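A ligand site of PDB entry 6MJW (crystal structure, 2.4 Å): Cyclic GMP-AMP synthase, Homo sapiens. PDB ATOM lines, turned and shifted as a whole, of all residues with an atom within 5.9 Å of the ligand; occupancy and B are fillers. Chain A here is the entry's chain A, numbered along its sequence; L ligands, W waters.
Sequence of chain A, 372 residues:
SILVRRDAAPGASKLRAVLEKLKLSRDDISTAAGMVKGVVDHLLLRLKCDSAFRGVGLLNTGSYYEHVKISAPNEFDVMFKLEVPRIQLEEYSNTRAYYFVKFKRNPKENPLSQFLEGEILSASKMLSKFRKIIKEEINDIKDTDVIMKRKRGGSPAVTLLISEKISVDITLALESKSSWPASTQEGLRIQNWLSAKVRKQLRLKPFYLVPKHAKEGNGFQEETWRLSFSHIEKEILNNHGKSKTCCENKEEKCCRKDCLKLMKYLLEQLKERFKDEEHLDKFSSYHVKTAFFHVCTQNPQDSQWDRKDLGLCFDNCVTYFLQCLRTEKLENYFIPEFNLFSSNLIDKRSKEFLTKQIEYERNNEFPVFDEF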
ATOM      1  N   VAL A  68     -25.597 -13.685  -3.756  1.00  0.00           N
ATOM      2  CA  VAL A  68     -26.314 -14.214  -4.908  1.00  0.00           C
ATOM      3  C   VAL A  68     -27.776 -14.505  -4.579  1.00  0.00           C
ATOM      4  O   VAL A  68     -28.653 -14.376  -5.453  1.00  0.00           O
ATOM      5  CB  VAL A  68     -25.555 -15.456  -5.398  1.00  0.00           C
ATOM      6  CG1 VAL A  68     -26.434 -16.360  -6.238  1.00  0.00           C
ATOM      7  CG2 VAL A  68     -24.297 -15.050  -6.174  1.00  0.00           C
ATOM      8  N   ALA A  97     -11.574 -13.166 -20.332  1.00  0.00           N
ATOM      9  CA  ALA A  97     -11.810 -12.651 -18.994  1.00  0.00           C
ATOM     10  C   ALA A  97     -10.669 -12.859 -18.014  1.00  0.00           C
ATOM     11  O   ALA A  97     -10.581 -12.131 -17.030  1.00  0.00           O
ATOM     12  CB  ALA A  97     -13.079 -13.282 -18.401  1.00  0.00           C
ATOM     13  N   TYR A  98      -9.788 -13.830 -18.256  1.00  0.00           N
ATOM     14  CA  TYR A  98      -8.715 -14.172 -17.326  1.00  0.00           C
ATOM     15  C   TYR A  98      -7.393 -13.577 -17.793  1.00  0.00           C
ATOM     16  O   TYR A  98      -7.087 -13.575 -18.991  1.00  0.00           O
ATOM     17  CB  TYR A  98      -8.585 -15.679 -17.164  1.00  0.00           C
ATOM     18  CG  TYR A  98      -9.824 -16.329 -16.608  1.00  0.00           C
ATOM     19  CD1 TYR A  98      -9.991 -16.500 -15.240  1.00  0.00           C
ATOM     20  CD2 TYR A  98     -10.839 -16.775 -17.449  1.00  0.00           C
ATOM     21  CE1 TYR A  98     -11.126 -17.102 -14.720  1.00  0.00           C
ATOM     22  CE2 TYR A  98     -11.971 -17.371 -16.937  1.00  0.00           C
ATOM     23  CZ  TYR A  98     -12.113 -17.532 -15.577  1.00  0.00           C
ATOM     24  OH  TYR A  98     -13.245 -18.129 -15.065  1.00  0.00           O
ATOM     25  N   SER A 155     -12.726 -16.941  -5.707  1.00  0.00           N
ATOM     26  CA  SER A 155     -13.781 -15.959  -5.939  1.00  0.00           C
ATOM     27  C   SER A 155     -14.315 -15.401  -4.631  1.00  0.00           C
ATOM     28  O   SER A 155     -14.355 -14.171  -4.485  1.00  0.00           O
ATOM     29  CB  SER A 155     -14.893 -16.569  -6.812  1.00  0.00           C
ATOM     30  OG  SER A 155     -15.937 -15.631  -7.016  1.00  0.00           O
ATOM     31  N   ARG A 226      -9.680 -12.573 -12.851  1.00  0.00           N
ATOM     32  CA  ARG A 226     -10.887 -12.397 -13.642  1.00  0.00           C
ATOM     33  C   ARG A 226     -11.360 -10.958 -13.544  1.00  0.00           C
ATOM     34  O   ARG A 226     -11.300 -10.343 -12.466  1.00  0.00           O
ATOM     35  CB  ARG A 226     -11.981 -13.344 -13.168  1.00  0.00           C
ATOM     36  CG  ARG A 226     -12.839 -13.911 -14.280  1.00  0.00           C
ATOM     37  CD  ARG A 226     -14.305 -13.621 -14.055  1.00  0.00           C
ATOM     38  NE  ARG A 226     -14.812 -14.164 -12.792  1.00  0.00           N
ATOM     39  CZ  ARG A 226     -15.183 -13.412 -11.757  1.00  0.00           C
ATOM     40  NH1 ARG A 226     -15.112 -12.086 -11.830  1.00  0.00           N
ATOM     41  NH2 ARG A 226     -15.627 -13.977 -10.644  1.00  0.00           N
ATOM     42  N   LEU A 227     -11.823 -10.402 -14.662  1.00  0.00           N
ATOM     43  CA  LEU A 227     -12.366  -9.064 -14.658  1.00  0.00           C
ATOM     44  C   LEU A 227     -13.671  -9.021 -13.862  1.00  0.00           C
ATOM     45  O   LEU A 227     -14.428  -9.995 -13.810  1.00  0.00           O
ATOM     46  CB  LEU A 227     -12.618  -8.579 -16.092  1.00  0.00           C
ATOM     47  CG  LEU A 227     -11.375  -8.426 -16.970  1.00  0.00           C
ATOM     48  CD1 LEU A 227     -11.755  -8.147 -18.412  1.00  0.00           C
ATOM     49  CD2 LEU A 227     -10.488  -7.316 -16.426  1.00  0.00           C
ATOM     50  N   SER A 228     -13.920  -7.877 -13.220  1.00  0.00           N
ATOM     51  CA  SER A 228     -15.125  -7.693 -12.417  1.00  0.00           C
ATOM     52  C   SER A 228     -15.681  -6.299 -12.650  1.00  0.00           C
ATOM     53  O   SER A 228     -14.939  -5.311 -12.623  1.00  0.00           O
ATOM     54  CB  SER A 228     -14.815  -7.889 -10.929  1.00  0.00           C
ATOM     55  OG  SER A 228     -15.931  -7.506 -10.126  1.00  0.00           O
ATOM     56  N   PHE A 229     -17.007  -6.216 -12.857  1.00  0.00           N
ATOM     57  CA  PHE A 229     -17.673  -4.930 -13.055  1.00  0.00           C
ATOM     58  C   PHE A 229     -18.871  -4.785 -12.122  1.00  0.00           C
ATOM     59  O   PHE A 229     -19.880  -4.168 -12.498  1.00  0.00           O
ATOM     60  CB  PHE A 229     -18.097  -4.761 -14.510  1.00  0.00           C
ATOM     61  CG  PHE A 229     -16.956  -4.766 -15.480  1.00  0.00           C
ATOM     62  CD1 PHE A 229     -16.274  -3.593 -15.769  1.00  0.00           C
ATOM     63  CD2 PHE A 229     -16.564  -5.941 -16.091  1.00  0.00           C
ATOM     64  CE1 PHE A 229     -15.222  -3.601 -16.668  1.00  0.00           C
ATOM     65  CE2 PHE A 229     -15.506  -5.953 -16.978  1.00  0.00           C
ATOM     66  CZ  PHE A 229     -14.834  -4.781 -17.270  1.00  0.00           C
ATOM     67  N   SER A 230     -18.769  -5.324 -10.902  1.00  0.00           N
ATOM     68  CA  SER A 230     -19.911  -5.296  -9.979  1.00  0.00           C
ATOM     69  C   SER A 230     -20.379  -3.874  -9.702  1.00  0.00           C
ATOM     70  O   SER A 230     -21.582  -3.615  -9.632  1.00  0.00           O
ATOM     71  CB  SER A 230     -19.531  -5.992  -8.672  1.00  0.00           C
ATOM     72  OG  SER A 230     -19.059  -7.298  -8.901  1.00  0.00           O
ATOM     73  N   GLU A 233     -22.485  -2.757 -12.557  1.00  0.00           N
ATOM     74  CA  GLU A 233     -23.775  -3.430 -12.566  1.00  0.00           C
ATOM     75  C   GLU A 233     -24.715  -2.835 -11.528  1.00  0.00           C
ATOM     76  O   GLU A 233     -25.913  -2.706 -11.776  1.00  0.00           O
ATOM     77  CB  GLU A 233     -23.564  -4.921 -12.320  1.00  0.00           C
ATOM     78  CG  GLU A 233     -22.809  -5.620 -13.443  1.00  0.00           C
ATOM     79  CD  GLU A 233     -22.114  -6.890 -12.983  1.00  0.00           C
ATOM     80  OE1 GLU A 233     -22.267  -7.275 -11.805  1.00  0.00           O
ATOM     81  OE2 GLU A 233     -21.406  -7.507 -13.810  1.00  0.00           O
ATOM     82  N   LYS A 282     -23.816 -25.279 -11.654  1.00  0.00           N
ATOM     83  CA  LYS A 282     -23.099 -24.229 -12.419  1.00  0.00           C
ATOM     84  C   LYS A 282     -23.833 -22.889 -12.437  1.00  0.00           C
ATOM     85  O   LYS A 282     -23.168 -21.862 -12.370  1.00  0.00           O
ATOM     86  CB  LYS A 282     -22.961 -24.662 -13.888  1.00  0.00           C
ATOM     87  CG  LYS A 282     -22.472 -26.078 -14.115  1.00  0.00           C
ATOM     88  CD  LYS A 282     -21.105 -26.384 -13.550  1.00  0.00           C
ATOM     89  CE  LYS A 282     -20.631 -27.762 -13.935  1.00  0.00           C
ATOM     90  NZ  LYS A 282     -19.151 -27.860 -13.908  1.00  0.00           N
ATOM     91  N   SER A 284     -25.887 -19.546 -11.599  1.00  0.00           N
ATOM     92  CA  SER A 284     -25.894 -18.609 -10.489  1.00  0.00           C
ATOM     93  C   SER A 284     -26.740 -17.393 -10.860  1.00  0.00           C
ATOM     94  O   SER A 284     -27.238 -17.279 -11.991  1.00  0.00           O
ATOM     95  CB  SER A 284     -24.473 -18.188 -10.100  1.00  0.00           C
ATOM     96  OG  SER A 284     -23.853 -17.474 -11.155  1.00  0.00           O
ATOM     97  N   SER A 285     -26.906 -16.486  -9.901  1.00  0.00           N
ATOM     98  CA  SER A 285     -27.657 -15.257 -10.171  1.00  0.00           C
ATOM     99  C   SER A 285     -26.951 -14.358 -11.174  1.00  0.00           C
ATOM    100  O   SER A 285     -27.584 -13.454 -11.721  1.00  0.00           O
ATOM    101  CB  SER A 285     -27.896 -14.490  -8.879  1.00  0.00           C
ATOM    102  OG  SER A 285     -26.674 -13.947  -8.389  1.00  0.00           O
ATOM    103  N   TYR A 286     -25.657 -14.575 -11.416  1.00  0.00           N
ATOM    104  CA  TYR A 286     -24.973 -13.767 -12.410  1.00  0.00           C
ATOM    105  C   TYR A 286     -25.489 -14.060 -13.803  1.00  0.00           C
ATOM    106  O   TYR A 286     -25.593 -13.155 -14.644  1.00  0.00           O
ATOM    107  CB  TYR A 286     -23.463 -13.995 -12.337  1.00  0.00           C
ATOM    108  CG  TYR A 286     -22.687 -12.972 -13.130  1.00  0.00           C
ATOM    109  CD1 TYR A 286     -22.659 -11.645 -12.717  1.00  0.00           C
ATOM    110  CD2 TYR A 286     -22.011 -13.317 -14.293  1.00  0.00           C
ATOM    111  CE1 TYR A 286     -21.959 -10.692 -13.437  1.00  0.00           C
ATOM    112  CE2 TYR A 286     -21.320 -12.364 -15.017  1.00  0.00           C
ATOM    113  CZ  TYR A 286     -21.303 -11.053 -14.580  1.00  0.00           C
ATOM    114  OH  TYR A 286     -20.608 -10.096 -15.287  1.00  0.00           O
ATOM    115  N   HIS A 287     -25.826 -15.322 -14.086  1.00  0.00           N
ATOM    116  CA  HIS A 287     -26.407 -15.658 -15.384  1.00  0.00           C
ATOM    117  C   HIS A 287     -27.762 -14.990 -15.554  1.00  0.00           C
ATOM    118  O   HIS A 287     -28.083 -14.480 -16.637  1.00  0.00           O
ATOM    119  CB  HIS A 287     -26.528 -17.178 -15.530  1.00  0.00           C
ATOM    120  CG  HIS A 287     -25.217 -17.896 -15.448  1.00  0.00           C
ATOM    121  ND1 HIS A 287     -24.825 -18.600 -14.329  1.00  0.00           N
ATOM    122  CD2 HIS A 287     -24.207 -18.024 -16.340  1.00  0.00           C
ATOM    123  CE1 HIS A 287     -23.628 -19.124 -14.541  1.00  0.00           C
ATOM    124  NE2 HIS A 287     -23.233 -18.788 -15.756  1.00  0.00           N
ATOM    125  N   ASN A 332     -21.437 -12.524 -21.855  1.00  0.00           N
ATOM    126  CA  ASN A 332     -21.175 -11.599 -20.771  1.00  0.00           C
ATOM    127  C   ASN A 332     -21.517 -10.184 -21.223  1.00  0.00           C
ATOM    128  O   ASN A 332     -21.188  -9.770 -22.330  1.00  0.00           O
ATOM    129  CB  ASN A 332     -19.711 -11.669 -20.343  1.00  0.00           C
ATOM    130  CG  ASN A 332     -19.429 -10.851 -19.103  1.00  0.00           C
ATOM    131  OD1 ASN A 332     -19.284  -9.628 -19.157  1.00  0.00           O
ATOM    132  ND2 ASN A 332     -19.362 -11.524 -17.957  1.00  0.00           N
ATOM    133  N   PHE A 334     -20.457  -7.321 -20.389  1.00  0.00           N
ATOM    134  CA  PHE A 334     -19.327  -6.432 -20.606  1.00  0.00           C
ATOM    135  C   PHE A 334     -18.288  -7.010 -21.551  1.00  0.00           C
ATOM    136  O   PHE A 334     -17.524  -6.248 -22.148  1.00  0.00           O
ATOM    137  CB  PHE A 334     -18.657  -6.105 -19.261  1.00  0.00           C
ATOM    138  CG  PHE A 334     -19.578  -5.458 -18.270  1.00  0.00           C
ATOM    139  CD1 PHE A 334     -20.425  -6.226 -17.500  1.00  0.00           C
ATOM    140  CD2 PHE A 334     -19.588  -4.086 -18.111  1.00  0.00           C
ATOM    141  CE1 PHE A 334     -21.281  -5.634 -16.591  1.00  0.00           C
ATOM    142  CE2 PHE A 334     -20.444  -3.495 -17.202  1.00  0.00           C
ATOM    143  CZ  PHE A 334     -21.285  -4.266 -16.443  1.00  0.00           C
ATOM    144  N   ILE A 335     -18.242  -8.330 -21.700  1.00  0.00           N
ATOM    145  CA  ILE A 335     -17.293  -8.987 -22.585  1.00  0.00           C
ATOM    146  C   ILE A 335     -18.080  -9.895 -23.525  1.00  0.00           C
ATOM    147  O   ILE A 335     -18.369 -11.051 -23.178  1.00  0.00           O
ATOM    148  CB  ILE A 335     -16.250  -9.788 -21.792  1.00  0.00           C
ATOM    149  CG1 ILE A 335     -15.654  -8.917 -20.682  1.00  0.00           C
ATOM    150  CG2 ILE A 335     -15.155 -10.287 -22.701  1.00  0.00           C
ATOM    151  CD1 ILE A 335     -14.598  -9.601 -19.886  1.00  0.00           C
ATOM    152  N   PHE A 338     -17.008 -13.711 -24.199  1.00  0.00           N
ATOM    153  CA  PHE A 338     -17.041 -14.686 -23.110  1.00  0.00           C
ATOM    154  C   PHE A 338     -18.447 -15.267 -23.025  1.00  0.00           C
ATOM    155  O   PHE A 338     -19.357 -14.642 -22.496  1.00  0.00           O
ATOM    156  CB  PHE A 338     -16.628 -14.049 -21.798  1.00  0.00           C
ATOM    157  CG  PHE A 338     -16.326 -15.041 -20.710  1.00  0.00           C
ATOM    158  CD1 PHE A 338     -17.308 -15.435 -19.817  1.00  0.00           C
ATOM    159  CD2 PHE A 338     -15.049 -15.574 -20.578  1.00  0.00           C
ATOM    160  CE1 PHE A 338     -17.024 -16.354 -18.817  1.00  0.00           C
ATOM    161  CE2 PHE A 338     -14.764 -16.479 -19.581  1.00  0.00           C
ATOM    162  CZ  PHE A 338     -15.751 -16.869 -18.701  1.00  0.00           C
ATOM    163  N   LEU A 340     -20.972 -17.355 -21.303  1.00  0.00           N
ATOM    164  CA  LEU A 340     -21.210 -17.982 -20.012  1.00  0.00           C
ATOM    165  C   LEU A 340     -21.881 -19.349 -20.142  1.00  0.00           C
ATOM    166  O   LEU A 340     -21.776 -20.166 -19.220  1.00  0.00           O
ATOM    167  CB  LEU A 340     -22.066 -17.072 -19.142  1.00  0.00           C
ATOM    168  CG  LEU A 340     -21.462 -15.701 -18.850  1.00  0.00           C
ATOM    169  CD1 LEU A 340     -22.547 -14.736 -18.413  1.00  0.00           C
ATOM    170  CD2 LEU A 340     -20.391 -15.800 -17.782  1.00  0.00           C
ATOM    171  N   LEU A 345     -17.745 -24.328 -19.845  1.00  0.00           N
ATOM    172  CA  LEU A 345     -18.066 -23.945 -18.476  1.00  0.00           C
ATOM    173  C   LEU A 345     -19.237 -24.743 -17.906  1.00  0.00           C
ATOM    174  O   LEU A 345     -19.218 -25.094 -16.719  1.00  0.00           O
ATOM    175  CB  LEU A 345     -18.380 -22.453 -18.414  1.00  0.00           C
ATOM    176  CG  LEU A 345     -17.231 -21.502 -18.747  1.00  0.00           C
ATOM    177  CD1 LEU A 345     -17.723 -20.065 -18.748  1.00  0.00           C
ATOM    178  CD2 LEU A 345     -16.075 -21.664 -17.757  1.00  0.00           C
HETATM  179  C1  LIG L   1     -19.273 -13.683  -9.972  1.00  0.00           C
HETATM  180  C2  LIG L   1     -17.493 -15.710 -15.033  1.00  0.00           C
HETATM  181  C3  LIG L   1     -16.337 -16.355 -15.377  1.00  0.00           C
HETATM  182  C4  LIG L   1     -18.629 -16.448 -14.775  1.00  0.00           C
HETATM  183  O1  LIG L   1     -21.306 -16.850  -8.038  1.00  0.00           O
HETATM  184  C5  LIG L   1     -21.256 -15.642  -8.748  1.00  0.00           C
HETATM  185  C6  LIG L   1     -20.608 -15.831 -10.128  1.00  0.00           C
HETATM  186  O2  LIG L   1     -20.877 -16.764 -10.779  1.00  0.00           O
HETATM  187  N1  LIG L   1     -19.673 -14.875 -10.666  1.00  0.00           N
HETATM  188  C7  LIG L   1     -19.059 -15.063 -11.998  1.00  0.00           C
HETATM  189  C8  LIG L   1     -18.641 -13.727 -12.704  1.00  0.00           C
HETATM  190  C9  LIG L   1     -17.987 -13.417 -13.946  1.00  0.00           C
HETATM  191  C10 LIG L   1     -17.897 -12.063 -14.018  1.00  0.00           C
HETATM  192  N2  LIG L   1     -18.464 -11.552 -12.892  1.00  0.00           N
HETATM  193  C11 LIG L   1     -18.922 -12.566 -12.116  1.00  0.00           C
HETATM  194  C12 LIG L   1     -19.594 -12.485 -10.789  1.00  0.00           C
HETATM  195  C13 LIG L   1     -17.290 -11.464 -15.126  1.00  0.00           C
HETATM  196 CL1  LIG L   1     -17.127  -9.714 -15.372  1.00  0.00          CL
HETATM  197  C14 LIG L   1     -16.784 -12.234 -16.138  1.00  0.00           C
HETATM  198 CL2  LIG L   1     -16.033 -11.419 -17.526  1.00  0.00          CL
HETATM  199  C15 LIG L   1     -16.855 -13.608 -16.083  1.00  0.00           C
HETATM  200  C16 LIG L   1     -17.460 -14.193 -15.003  1.00  0.00           C
HETATM  201  N3  LIG L   1     -16.280 -17.659 -15.436  1.00  0.00           N
HETATM  202  C17 LIG L   1     -17.335 -18.404 -15.184  1.00  0.00           C
HETATM  203  N4  LIG L   1     -17.192 -19.844 -15.265  1.00  0.00           N
HETATM  204  C18 LIG L   1     -18.539 -17.816 -14.847  1.00  0.00           C
HETATM  205  O   HOH W   1     -18.627  -8.364 -12.951  1.00  0.00           O
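An oxygen (O2) of the ligand is in hydrogen-bond range of the side-chain hydroxyl (OG) of Ser 284, at 3.1 Å.
A nitrogen (N3) of the ligand is in hydrogen-bond range of the side-chain hydroxyl (OH) of Tyr 98 (3.1 Å).
The side-chain hydroxyl (OG) of Ser 284 sits close to the backbone NH (N) of Tyr 286.
N of Ser 284 is in hydrogen-bond range of ND1 of His 287 (3.1 Å).
The backbone NH of Leu 227 sits at hydrogen-bond distance from the backbone carbonyl oxygen of Ala 97.
OD1 of Asn 332 lies within hydrogen-bond range of N of Ile 335.
OH of Tyr 286 sits at hydrogen-bond distance from ND2 of Asn 332 (3.3 Å).
O of Phe 338 lies within hydrogen-bond range of N of Asn 332, at 3.0 Å.
N of Phe 334 is in hydrogen-bond range of OD1 of Asn 332.
The side-chain carboxylate of Glu 233 lies within hydrogen-bond range of the side-chain hydroxyl of Tyr 286 (3.1 Å).
Residues that only touch the ligand: Leu 227 (3.1 Å), Asn 332 (3.2 Å), Arg 226 (3.3 Å), Leu 345 (3.3 Å), Ile 335 (3.3 Å), Tyr 286 (3.3 Å), Phe 338 (3.4 Å), Leu 340 (3.5 Å), Ala 97 (3.6 Å), Phe 229 (3.9 Å) and Val 68 (3.96 Å).
Hydrophobic or aromatic side chains within 4 Å of the ligand: Val 68, Ala 97, Phe 229, Tyr 286, Ile 335, Phe 338, Leu 340 and Leu 345.
Within 4 Å of the ligand: Val 68, Ala 97, Tyr 98, Arg 226, Leu 227, Phe 229, Ser 284, Tyr 286, Asn 332, Ile 335, Phe 338, Leu 340 and Leu 345.
Water W1 lies within hydrogen-bond range of N of Phe 229, OE2 of Glu 233 and N2 of the ligand.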
